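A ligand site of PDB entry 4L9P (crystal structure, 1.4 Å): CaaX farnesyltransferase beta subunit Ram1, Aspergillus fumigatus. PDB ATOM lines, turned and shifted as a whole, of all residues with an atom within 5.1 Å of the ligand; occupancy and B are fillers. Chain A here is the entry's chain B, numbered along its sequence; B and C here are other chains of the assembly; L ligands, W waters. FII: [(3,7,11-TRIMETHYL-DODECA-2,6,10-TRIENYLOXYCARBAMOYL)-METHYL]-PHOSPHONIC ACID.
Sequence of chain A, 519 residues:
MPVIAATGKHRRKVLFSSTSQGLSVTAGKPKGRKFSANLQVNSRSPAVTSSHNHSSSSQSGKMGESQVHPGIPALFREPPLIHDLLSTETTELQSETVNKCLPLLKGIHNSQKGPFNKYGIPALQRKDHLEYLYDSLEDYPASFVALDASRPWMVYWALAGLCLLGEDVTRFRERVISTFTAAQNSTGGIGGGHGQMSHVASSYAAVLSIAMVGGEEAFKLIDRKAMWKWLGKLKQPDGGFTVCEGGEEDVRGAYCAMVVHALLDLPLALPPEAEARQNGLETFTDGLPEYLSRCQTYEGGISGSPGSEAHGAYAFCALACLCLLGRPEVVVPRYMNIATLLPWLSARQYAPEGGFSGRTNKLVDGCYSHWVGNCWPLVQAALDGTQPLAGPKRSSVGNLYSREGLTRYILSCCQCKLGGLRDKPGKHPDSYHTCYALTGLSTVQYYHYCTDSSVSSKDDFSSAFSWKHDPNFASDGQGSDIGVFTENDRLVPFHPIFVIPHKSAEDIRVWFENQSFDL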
ATOM      1  N   TRP A 153      -2.031 -25.796   1.712  1.00  0.00           N
ATOM      2  CA  TRP A 153      -2.538 -24.726   2.581  1.00  0.00           C
ATOM      3  C   TRP A 153      -4.049 -24.815   2.796  1.00  0.00           C
ATOM      4  O   TRP A 153      -4.534 -24.562   3.912  1.00  0.00           O
ATOM      5  CB  TRP A 153      -2.249 -23.348   2.011  1.00  0.00           C
ATOM      6  CG  TRP A 153      -0.875 -22.829   2.230  1.00  0.00           C
ATOM      7  CD1 TRP A 153      -0.023 -22.382   1.259  1.00  0.00           C
ATOM      8  CD2 TRP A 153      -0.248 -22.541   3.481  1.00  0.00           C
ATOM      9  NE1 TRP A 153       1.115 -21.866   1.839  1.00  0.00           N
ATOM     10  CE2 TRP A 153       1.004 -21.966   3.208  1.00  0.00           C
ATOM     11  CE3 TRP A 153      -0.642 -22.678   4.816  1.00  0.00           C
ATOM     12  CZ2 TRP A 153       1.884 -21.537   4.196  1.00  0.00           C
ATOM     13  CZ3 TRP A 153       0.262 -22.263   5.816  1.00  0.00           C
ATOM     14  CH2 TRP A 153       1.487 -21.700   5.484  1.00  0.00           C
ATOM     15  N   ALA A 201       6.593 -24.099   2.228  1.00  0.00           N
ATOM     16  CA  ALA A 201       5.253 -23.716   2.717  1.00  0.00           C
ATOM     17  C   ALA A 201       4.262 -24.869   2.616  1.00  0.00           C
ATOM     18  O   ALA A 201       3.442 -25.092   3.504  1.00  0.00           O
ATOM     19  CB  ALA A 201       4.747 -22.461   1.985  1.00  0.00           C
ATOM     20  N   TYR A 204       5.260 -27.305   5.333  1.00  0.00           N
ATOM     21  CA  TYR A 204       4.766 -26.843   6.627  1.00  0.00           C
ATOM     22  C   TYR A 204       3.258 -27.124   6.743  1.00  0.00           C
ATOM     23  O   TYR A 204       2.783 -27.683   7.737  1.00  0.00           O
ATOM     24  CB  TYR A 204       5.089 -25.352   6.664  1.00  0.00           C
ATOM     25  CG  TYR A 204       4.428 -24.543   7.763  1.00  0.00           C
ATOM     26  CD1 TYR A 204       5.062 -24.312   8.986  1.00  0.00           C
ATOM     27  CD2 TYR A 204       3.183 -23.928   7.561  1.00  0.00           C
ATOM     28  CE1 TYR A 204       4.501 -23.491   9.976  1.00  0.00           C
ATOM     29  CE2 TYR A 204       2.621 -23.083   8.506  1.00  0.00           C
ATOM     30  CZ  TYR A 204       3.287 -22.873   9.715  1.00  0.00           C
ATOM     31  OH  TYR A 204       2.689 -22.034  10.626  1.00  0.00           O
ATOM     32  N   ARG A 252       9.957 -16.464   5.579  1.00  0.00           N
ATOM     33  CA  ARG A 252       9.050 -17.628   5.471  1.00  0.00           C
ATOM     34  C   ARG A 252       9.814 -18.888   5.318  1.00  0.00           C
ATOM     35  O   ARG A 252       9.438 -19.920   5.907  1.00  0.00           O
ATOM     36  CB  ARG A 252       8.191 -17.635   4.177  1.00  0.00           C
ATOM     37  CG  ARG A 252       7.298 -16.531   4.183  1.00  0.00           C
ATOM     38  CD  ARG A 252       6.573 -16.572   2.736  1.00  0.00           C
ATOM     39  NE  ARG A 252       7.543 -16.379   1.669  1.00  0.00           N
ATOM     40  CZ  ARG A 252       7.488 -16.988   0.467  1.00  0.00           C
ATOM     41  NH1 ARG A 252       6.504 -17.806   0.111  1.00  0.00           N
ATOM     42  NH2 ARG A 252       8.423 -16.748  -0.355  1.00  0.00           N
ATOM     43  N   TYR A 255      11.291 -19.800   8.821  1.00  0.00           N
ATOM     44  CA  TYR A 255      10.303 -20.254   9.801  1.00  0.00           C
ATOM     45  C   TYR A 255       9.666 -21.581   9.377  1.00  0.00           C
ATOM     46  O   TYR A 255       9.555 -22.543  10.192  1.00  0.00           O
ATOM     47  CB  TYR A 255       9.206 -19.175   9.906  1.00  0.00           C
ATOM     48  CG  TYR A 255       7.983 -19.637  10.622  1.00  0.00           C
ATOM     49  CD1 TYR A 255       7.979 -19.868  12.003  1.00  0.00           C
ATOM     50  CD2 TYR A 255       6.810 -19.859   9.900  1.00  0.00           C
ATOM     51  CE1 TYR A 255       6.824 -20.354  12.632  1.00  0.00           C
ATOM     52  CE2 TYR A 255       5.672 -20.315  10.503  1.00  0.00           C
ATOM     53  CZ  TYR A 255       5.674 -20.583  11.881  1.00  0.00           C
ATOM     54  OH  TYR A 255       4.523 -21.082  12.461  1.00  0.00           O
ATOM     55  N   CYS A 256       9.236 -21.715   8.112  1.00  0.00           N
ATOM     56  CA  CYS A 256       8.597 -22.965   7.703  1.00  0.00           C
ATOM     57  C   CYS A 256       9.571 -24.148   7.748  1.00  0.00           C
ATOM     58  O   CYS A 256       9.180 -25.230   8.206  1.00  0.00           O
ATOM     59  CB  CYS A 256       8.035 -22.846   6.290  1.00  0.00           C
ATOM     60  SG  CYS A 256       6.619 -21.699   6.134  1.00  0.00           S
ATOM     61  N   HIS A 311       7.245  -5.799   8.310  1.00  0.00           N
ATOM     62  CA  HIS A 311       5.884  -6.272   8.043  1.00  0.00           C
ATOM     63  C   HIS A 311       5.513  -7.289   9.110  1.00  0.00           C
ATOM     64  O   HIS A 311       6.283  -8.187   9.429  1.00  0.00           O
ATOM     65  CB  HIS A 311       5.824  -6.950   6.650  1.00  0.00           C
ATOM     66  CG  HIS A 311       4.438  -7.109   6.146  1.00  0.00           C
ATOM     67  ND1 HIS A 311       3.568  -8.069   6.645  1.00  0.00           N
ATOM     68  CD2 HIS A 311       3.753  -6.423   5.220  1.00  0.00           C
ATOM     69  CE1 HIS A 311       2.388  -7.928   6.050  1.00  0.00           C
ATOM     70  NE2 HIS A 311       2.486  -6.922   5.163  1.00  0.00           N
ATOM     71  N   ALA A 313       3.679  -9.986   9.016  1.00  0.00           N
ATOM     72  CA  ALA A 313       3.762 -11.389   8.699  1.00  0.00           C
ATOM     73  C   ALA A 313       5.189 -11.903   8.858  1.00  0.00           C
ATOM     74  O   ALA A 313       5.418 -13.022   9.347  1.00  0.00           O
ATOM     75  CB  ALA A 313       3.316 -11.607   7.297  1.00  0.00           C
ATOM     76  N   TYR A 314       6.147 -11.082   8.452  1.00  0.00           N
ATOM     77  CA  TYR A 314       7.552 -11.505   8.531  1.00  0.00           C
ATOM     78  C   TYR A 314       8.081 -11.345   9.954  1.00  0.00           C
ATOM     79  O   TYR A 314       8.950 -12.129  10.384  1.00  0.00           O
ATOM     80  CB  TYR A 314       8.376 -10.701   7.550  1.00  0.00           C
ATOM     81  CG  TYR A 314       7.978 -11.001   6.111  1.00  0.00           C
ATOM     82  CD1 TYR A 314       7.937 -12.323   5.635  1.00  0.00           C
ATOM     83  CD2 TYR A 314       7.807  -9.985   5.144  1.00  0.00           C
ATOM     84  CE1 TYR A 314       7.679 -12.611   4.280  1.00  0.00           C
ATOM     85  CE2 TYR A 314       7.539 -10.290   3.813  1.00  0.00           C
ATOM     86  CZ  TYR A 314       7.479 -11.564   3.380  1.00  0.00           C
ATOM     87  OH  TYR A 314       7.276 -11.810   2.039  1.00  0.00           O
ATOM     88  N   CYS A 317       7.103 -14.631  11.501  1.00  0.00           N
ATOM     89  CA  CYS A 317       8.015 -15.726  11.096  1.00  0.00           C
ATOM     90  C   CYS A 317       9.373 -15.642  11.820  1.00  0.00           C
ATOM     91  O   CYS A 317       9.905 -16.668  12.264  1.00  0.00           O
ATOM     92  CB  CYS A 317       8.276 -15.629   9.579  1.00  0.00           C
ATOM     93  SG  CYS A 317       6.840 -16.085   8.561  1.00  0.00           S
ATOM     94  N   GLY A 358      -0.562  -4.623   8.748  1.00  0.00           N
ATOM     95  CA  GLY A 358       0.729  -5.342   8.593  1.00  0.00           C
ATOM     96  C   GLY A 358       1.948  -4.481   8.537  1.00  0.00           C
ATOM     97  O   GLY A 358       3.040  -4.906   8.811  1.00  0.00           O
ATOM     98  N   ARG A 359       1.753  -3.236   8.125  1.00  0.00           N
ATOM     99  CA  ARG A 359       2.888  -2.298   7.972  1.00  0.00           C
ATOM    100  C   ARG A 359       2.408  -0.876   8.046  1.00  0.00           C
ATOM    101  O   ARG A 359       1.194  -0.589   7.932  1.00  0.00           O
ATOM    102  CB  ARG A 359       3.694  -2.562   6.660  1.00  0.00           C
ATOM    103  CG  ARG A 359       2.791  -2.800   5.463  1.00  0.00           C
ATOM    104  CD  ARG A 359       3.706  -2.963   4.176  1.00  0.00           C
ATOM    105  NE  ARG A 359       2.942  -3.585   3.112  1.00  0.00           N
ATOM    106  CZ  ARG A 359       3.144  -3.312   1.811  1.00  0.00           C
ATOM    107  NH1 ARG A 359       4.175  -2.526   1.418  1.00  0.00           N
ATOM    108  NH2 ARG A 359       2.354  -3.888   0.927  1.00  0.00           N
ATOM    109  N   LYS A 362      -0.585   1.274   6.201  1.00  0.00           N
ATOM    110  CA  LYS A 362      -1.505   0.436   5.423  1.00  0.00           C
ATOM    111  C   LYS A 362      -2.701   0.052   6.297  1.00  0.00           C
ATOM    112  O   LYS A 362      -2.874   0.659   7.374  1.00  0.00           O
ATOM    113  CB  LYS A 362      -0.772  -0.773   4.796  1.00  0.00           C
ATOM    114  CG  LYS A 362       0.284  -0.298   3.756  1.00  0.00           C
ATOM    115  CD  LYS A 362       0.503  -1.291   2.672  1.00  0.00           C
ATOM    116  CE  LYS A 362      -0.626  -1.203   1.668  1.00  0.00           C
ATOM    117  NZ  LYS A 362      -0.673  -2.364   0.719  1.00  0.00           N
ATOM    118  N   LEU A 363      -3.537  -0.849   5.829  1.00  0.00           N
ATOM    119  CA  LEU A 363      -4.871  -0.992   6.454  1.00  0.00           C
ATOM    120  C   LEU A 363      -4.911  -2.206   7.365  1.00  0.00           C
ATOM    121  O   LEU A 363      -4.210  -3.205   7.186  1.00  0.00           O
ATOM    122  CB  LEU A 363      -5.899  -1.214   5.348  1.00  0.00           C
ATOM    123  CG  LEU A 363      -6.007  -0.102   4.291  1.00  0.00           C
ATOM    124  CD1 LEU A 363      -7.019  -0.489   3.215  1.00  0.00           C
ATOM    125  CD2 LEU A 363      -6.399   1.216   4.944  1.00  0.00           C
ATOM    126  N   ASP A 365      -6.386  -5.756   8.745  1.00  0.00           N
ATOM    127  CA  ASP A 365      -6.822  -6.968   8.055  1.00  0.00           C
ATOM    128  C   ASP A 365      -6.884  -8.085   9.094  1.00  0.00           C
ATOM    129  O   ASP A 365      -5.962  -8.259   9.911  1.00  0.00           O
ATOM    130  CB  ASP A 365      -5.753  -7.279   6.941  1.00  0.00           C
ATOM    131  CG  ASP A 365      -5.930  -8.566   6.253  1.00  0.00           C
ATOM    132  OD1 ASP A 365      -6.691  -9.473   6.673  1.00  0.00           O
ATOM    133  OD2 ASP A 365      -5.315  -8.745   5.191  1.00  0.00           O
ATOM    134  N   TYR A 368      -4.045 -10.554  10.163  1.00  0.00           N
ATOM    135  CA  TYR A 368      -2.977 -10.121  11.083  1.00  0.00           C
ATOM    136  C   TYR A 368      -3.385 -10.397  12.539  1.00  0.00           C
ATOM    137  O   TYR A 368      -2.558 -10.244  13.416  1.00  0.00           O
ATOM    138  CB  TYR A 368      -2.577  -8.637  10.863  1.00  0.00           C
ATOM    139  CG  TYR A 368      -2.043  -8.427   9.431  1.00  0.00           C
ATOM    140  CD1 TYR A 368      -1.098  -9.326   8.912  1.00  0.00           C
ATOM    141  CD2 TYR A 368      -2.556  -7.439   8.633  1.00  0.00           C
ATOM    142  CE1 TYR A 368      -0.630  -9.203   7.560  1.00  0.00           C
ATOM    143  CE2 TYR A 368      -2.115  -7.272   7.313  1.00  0.00           C
ATOM    144  CZ  TYR A 368      -1.190  -8.191   6.809  1.00  0.00           C
ATOM    145  OH  TYR A 368      -0.724  -8.046   5.511  1.00  0.00           O
ATOM    146  N   TRP A 371      -0.921 -12.998  12.509  1.00  0.00           N
ATOM    147  CA  TRP A 371       0.525 -12.714  12.270  1.00  0.00           C
ATOM    148  C   TRP A 371       1.042 -11.679  13.270  1.00  0.00           C
ATOM    149  O   TRP A 371       2.171 -11.829  13.757  1.00  0.00           O
ATOM    150  CB  TRP A 371       0.750 -12.190  10.836  1.00  0.00           C
ATOM    151  CG  TRP A 371       0.289 -13.179   9.780  1.00  0.00           C
ATOM    152  CD1 TRP A 371      -0.756 -13.018   8.892  1.00  0.00           C
ATOM    153  CD2 TRP A 371       0.804 -14.484   9.545  1.00  0.00           C
ATOM    154  NE1 TRP A 371      -0.924 -14.142   8.123  1.00  0.00           N
ATOM    155  CE2 TRP A 371       0.023 -15.078   8.499  1.00  0.00           C
ATOM    156  CE3 TRP A 371       1.849 -15.210  10.089  1.00  0.00           C
ATOM    157  CZ2 TRP A 371       0.239 -16.381   8.037  1.00  0.00           C
ATOM    158  CZ3 TRP A 371       2.070 -16.507   9.650  1.00  0.00           C
ATOM    159  CH2 TRP A 371       1.274 -17.067   8.597  1.00  0.00           C
ATOM    160  N   TYR A 432      -8.350 -18.944   4.339  1.00  0.00           N
ATOM    161  CA  TYR A 432      -7.121 -18.342   4.934  1.00  0.00           C
ATOM    162  C   TYR A 432      -7.527 -17.295   5.976  1.00  0.00           C
ATOM    163  O   TYR A 432      -7.035 -17.338   7.142  1.00  0.00           O
ATOM    164  CB  TYR A 432      -6.250 -17.726   3.821  1.00  0.00           C
ATOM    165  CG  TYR A 432      -5.215 -16.750   4.258  1.00  0.00           C
ATOM    166  CD1 TYR A 432      -3.914 -17.179   4.636  1.00  0.00           C
ATOM    167  CD2 TYR A 432      -5.510 -15.384   4.327  1.00  0.00           C
ATOM    168  CE1 TYR A 432      -2.970 -16.256   5.064  1.00  0.00           C
ATOM    169  CE2 TYR A 432      -4.556 -14.461   4.735  1.00  0.00           C
ATOM    170  CZ  TYR A 432      -3.292 -14.893   5.109  1.00  0.00           C
ATOM    171  OH  TYR A 432      -2.397 -13.937   5.573  1.00  0.00           O
ATOM    172  N   LYS B 121       0.683  -9.028  -6.814  1.00  0.00           N
ATOM    173  CA  LYS B 121       1.026  -9.870  -5.667  1.00  0.00           C
ATOM    174  C   LYS B 121       1.451 -11.283  -5.971  1.00  0.00           C
ATOM    175  O   LYS B 121       0.762 -12.272  -5.611  1.00  0.00           O
ATOM    176  CB  LYS B 121      -0.075  -9.918  -4.624  1.00  0.00           C
ATOM    177  CG  LYS B 121      -0.032  -8.764  -3.798  1.00  0.00           C
ATOM    178  CD  LYS B 121      -1.308  -8.715  -3.021  1.00  0.00           C
ATOM    179  CE  LYS B 121      -1.521  -7.375  -2.374  1.00  0.00           C
ATOM    180  NZ  LYS B 121      -2.882  -7.341  -1.941  1.00  0.00           N
ATOM    181  N   TYR B 123       4.918 -13.788  -5.953  1.00  0.00           N
ATOM    182  CA  TYR B 123       6.334 -14.027  -5.635  1.00  0.00           C
ATOM    183  C   TYR B 123       7.183 -14.457  -6.823  1.00  0.00           C
ATOM    184  O   TYR B 123       8.366 -14.043  -6.919  1.00  0.00           O
ATOM    185  CB  TYR B 123       6.449 -15.110  -4.584  1.00  0.00           C
ATOM    186  CG  TYR B 123       6.236 -14.653  -3.153  1.00  0.00           C
ATOM    187  CD1 TYR B 123       4.964 -14.680  -2.593  1.00  0.00           C
ATOM    188  CD2 TYR B 123       7.318 -14.156  -2.385  1.00  0.00           C
ATOM    189  CE1 TYR B 123       4.776 -14.335  -1.238  1.00  0.00           C
ATOM    190  CE2 TYR B 123       7.062 -13.770  -1.050  1.00  0.00           C
ATOM    191  CZ  TYR B 123       5.796 -13.862  -0.524  1.00  0.00           C
ATOM    192  OH  TYR B 123       5.545 -13.496   0.804  1.00  0.00           O
ATOM    193  N   TYR B 161       4.861  -4.771  -2.348  1.00  0.00           N
ATOM    194  CA  TYR B 161       5.997  -5.218  -1.542  1.00  0.00           C
ATOM    195  C   TYR B 161       6.996  -5.973  -2.377  1.00  0.00           C
ATOM    196  O   TYR B 161       8.230  -5.824  -2.155  1.00  0.00           O
ATOM    197  CB  TYR B 161       5.449  -6.162  -0.395  1.00  0.00           C
ATOM    198  CG  TYR B 161       6.420  -6.369   0.735  1.00  0.00           C
ATOM    199  CD1 TYR B 161       7.437  -7.314   0.642  1.00  0.00           C
ATOM    200  CD2 TYR B 161       6.352  -5.578   1.913  1.00  0.00           C
ATOM    201  CE1 TYR B 161       8.335  -7.531   1.703  1.00  0.00           C
ATOM    202  CE2 TYR B 161       7.232  -5.785   2.949  1.00  0.00           C
ATOM    203  CZ  TYR B 161       8.246  -6.749   2.814  1.00  0.00           C
ATOM    204  OH  TYR B 161       9.145  -6.977   3.840  1.00  0.00           O
ATOM    205  N   HIS B 162       6.541  -6.808  -3.320  1.00  0.00           N
ATOM    206  CA  HIS B 162       7.514  -7.616  -4.064  1.00  0.00           C
ATOM    207  C   HIS B 162       8.315  -6.746  -5.025  1.00  0.00           C
ATOM    208  O   HIS B 162       9.479  -7.064  -5.292  1.00  0.00           O
ATOM    209  CB  HIS B 162       6.750  -8.659  -4.860  1.00  0.00           C
ATOM    210  CG  HIS B 162       5.987  -9.608  -3.988  1.00  0.00           C
ATOM    211  ND1 HIS B 162       4.603  -9.743  -4.025  1.00  0.00           N
ATOM    212  CD2 HIS B 162       6.395 -10.278  -2.898  1.00  0.00           C
ATOM    213  CE1 HIS B 162       4.221 -10.587  -3.066  1.00  0.00           C
ATOM    214  NE2 HIS B 162       5.307 -10.964  -2.405  1.00  0.00           N
ATOM    215  N   LYS C   1      -6.693  -8.820  -1.134  1.00  0.00           N
ATOM    216  CA  LYS C   1      -6.184 -10.146  -1.504  1.00  0.00           C
ATOM    217  C   LYS C   1      -4.829 -10.417  -0.881  1.00  0.00           C
ATOM    218  O   LYS C   1      -3.895  -9.622  -1.047  1.00  0.00           O
ATOM    219  CB  LYS C   1      -6.004 -10.256  -2.999  1.00  0.00           C
ATOM    220  CG  LYS C   1      -5.940 -11.715  -3.438  1.00  0.00           C
ATOM    221  CD  LYS C   1      -4.755 -11.947  -4.318  1.00  0.00           C
ATOM    222  CE  LYS C   1      -5.026 -13.104  -5.269  1.00  0.00           C
ATOM    223  NZ  LYS C   1      -5.582 -14.279  -4.516  1.00  0.00           N
ATOM    224  N   VAL C   3      -1.552 -13.032  -0.193  1.00  0.00           N
ATOM    225  CA  VAL C   3      -0.835 -14.086  -0.885  1.00  0.00           C
ATOM    226  C   VAL C   3       0.259 -14.413   0.089  1.00  0.00           C
ATOM    227  O   VAL C   3       0.763 -13.507   0.695  1.00  0.00           O
ATOM    228  CB  VAL C   3      -0.258 -13.536  -2.190  1.00  0.00           C
ATOM    229  CG1 VAL C   3       0.803 -14.458  -2.840  1.00  0.00           C
ATOM    230  CG2 VAL C   3      -1.406 -13.271  -3.204  1.00  0.00           C
ATOM    231  N   VAL C   4       0.562 -15.708   0.259  1.00  0.00           N
ATOM    232  CA  VAL C   4       1.605 -16.200   1.146  1.00  0.00           C
ATOM    233  C   VAL C   4       2.693 -17.018   0.437  1.00  0.00           C
ATOM    234  O   VAL C   4       3.701 -17.325   1.058  1.00  0.00           O
ATOM    235  CB  VAL C   4       1.057 -17.036   2.317  1.00  0.00           C
ATOM    236  CG1 VAL C   4      -0.039 -16.282   2.994  1.00  0.00           C
ATOM    237  CG2 VAL C   4       0.453 -18.312   1.835  1.00  0.00           C
HETATM  238  C1  FII L   1       4.263 -18.941   7.194  1.00  0.00           C
HETATM  239  C2  FII L   1       3.976 -17.963   6.090  1.00  0.00           C
HETATM  240  C6  FII L   1       4.012 -18.515   4.725  1.00  0.00           C
HETATM  241  C10 FII L   1       4.083 -16.529   6.387  1.00  0.00           C
HETATM  242  C11 FII L   1       3.901 -15.420   5.351  1.00  0.00           C
HETATM  243  C12 FII L   1       2.450 -14.878   5.493  1.00  0.00           C
HETATM  244  C15 FII L   1       2.156 -13.502   4.901  1.00  0.00           C
HETATM  245  C18 FII L   1       0.752 -12.924   5.019  1.00  0.00           C
HETATM  246  C22 FII L   1       3.130 -13.017   3.884  1.00  0.00           C
HETATM  247  C23 FII L   1       3.053 -11.529   3.590  1.00  0.00           C
HETATM  248  C24 FII L   1       3.850 -11.156   2.397  1.00  0.00           C
HETATM  249  C27 FII L   1       3.417  -9.831   1.872  1.00  0.00           C
HETATM  250  C30 FII L   1       4.141  -8.629   2.455  1.00  0.00           C
HETATM  251  C34 FII L   1       2.906  -9.850   0.477  1.00  0.00           C
HETATM  252  C35 FII L   1       2.680  -8.590  -0.330  1.00  0.00           C
HETATM  253  O36 FII L   1       1.297  -8.392  -0.586  1.00  0.00           O
HETATM  254  N42 FII L   1       0.484  -8.355   0.509  1.00  0.00           N
HETATM  255  C43 FII L   1       0.139  -7.038   0.869  1.00  0.00           C
HETATM  256  O44 FII L   1       0.550  -6.009   0.309  1.00  0.00           O
HETATM  257  C45 FII L   1      -0.832  -6.991   2.038  1.00  0.00           C
HETATM  258  P46 FII L   1      -0.613  -5.500   3.147  1.00  0.00           P
HETATM  259  O49 FII L   1       0.845  -5.402   3.414  1.00  0.00           O
HETATM  260  O50 FII L   1      -1.228  -4.325   2.462  1.00  0.00           O
HETATM  261  O51 FII L   1      -1.414  -5.916   4.398  1.00  0.00           O
HETATM  262  O   HOH W   1       2.052  -5.488  -1.830  1.00  0.00           O
HETATM  263  O   HOH W   2      -1.612  -3.821   6.315  1.00  0.00           O
HETATM  264  O   HOH W   3      -3.288  -2.741   3.470  1.00  0.00           O
HETATM  265  O   HOH W   4      -4.115  -7.540   1.074  1.00  0.00           O
HETATM  266  O   HOH W   5      -3.365  -5.001   0.839  1.00  0.00           O
HETATM  267  O   HOH W   6      -0.403 -10.827   1.337  1.00  0.00           O
HETATM  268  O   HOH W   7      -2.193  -4.796  -1.355  1.00  0.00           O
HETATM  269  O   HOH W   8       1.710 -11.592  -2.045  1.00  0.00           O
HETATM  270  O   HOH W   9      -3.981  -6.753   3.934  1.00  0.00           O
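The side-chain hydroxyl (OH) of Tyr 368 is in hydrogen-bond range of an oxygen (O51) of the ligand, 2.5 Å away. NZ of Lys 362 lies within salt-bridge range of O50 of the ligand (2.7 Å). The guanidinium group of Arg 359 lies within salt-bridge range of an oxygen (O49) of the ligand. A ring nitrogen (NE2) of His 311 lies within hydrogen-bond range of an oxygen (O49) of the ligand (2.8 Å).
A ring nitrogen (NE2) of His 311 lies close to the side-chain hydroxyl (OH) of Tyr 368, at 3.4 Å. The backbone NH (N) of Ala 313 sits at hydrogen-bond distance from a ring nitrogen (ND1) of His 311 (3.1 Å). The backbone carbonyl oxygen (O) of Ala 313 sits at hydrogen-bond distance from the side-chain sulfur (SG) of Cys 317. The side-chain hydroxyl (OH) of Tyr 314 lies within hydrogen-bond range of the side-chain hydroxyl (OH) of Tyr 123 of chain B (2.7 Å). OH of Tyr 432 sits at hydrogen-bond distance from NE1 of Trp 371, 3.0 Å away. NZ of Lys 121 of chain B is in hydrogen-bond range of O of Lys 1 of chain C (2.7 Å). O of Arg 252 lies close to SG of Cys 256. The side-chain hydroxyl of Tyr 255 lies within hydrogen-bond range of the side-chain hydroxyl of Tyr 204, at 2.8 Å.
Merely in contact with the ligand: Trp 153 (3.7 Å), Arg 252 (3.8 Å), Tyr 255 (3.8 Å), Cys 256 (3.8 Å), Ala 313 (3.3 Å), Tyr 314 (3.5 Å), Cys 317 (3.5 Å), Trp 371 (3.6 Å), Tyr 432 (3.4 Å), Lys 121 of chain B (3.5 Å), Tyr 123 of chain B (3.3 Å), Tyr 161 of chain B (3.6 Å), His 162 of chain B (3.7 Å) and Val 4 of chain C (3.8 Å). Within 4 Å of the ligand: Trp 153, Arg 252, Tyr 255, Cys 256, His 311, Ala 313, Tyr 314, Cys 317, Arg 359, Lys 362, Tyr 368, Trp 371, Tyr 432, Lys 121 of chain B, Tyr 123 of chain B, Tyr 161 of chain B, His 162 of chain B and Val 4 of chain C.
Water W1 lies within hydrogen-bond range of an oxygen (O44) of the ligand, the backbone NH (N) of Tyr 161 of chain B and the guanidinium group (NH2) of Arg 359. Water W6 bridges a nitrogen (N42) of the ligand (2.8 Å) and the backbone NH (N) of Val 3 of chain C (2.9 Å). Water W3 lies within hydrogen-bond range of an oxygen (O50) of the ligand and the backbone NH (N) of Leu 363. Water W2 lies within hydrogen-bond range of N of Gly 358 (2.8 Å), O of Leu 363 (2.8 Å) and O51 of the ligand (2.8 Å). Water W7 bridges NZ of Lys 121 of chain B and O44 of the ligand. Water W4 bridges O of Lys 1 of chain C (3.0 Å) and NZ of Lys 121 of chain B (3.3 Å).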
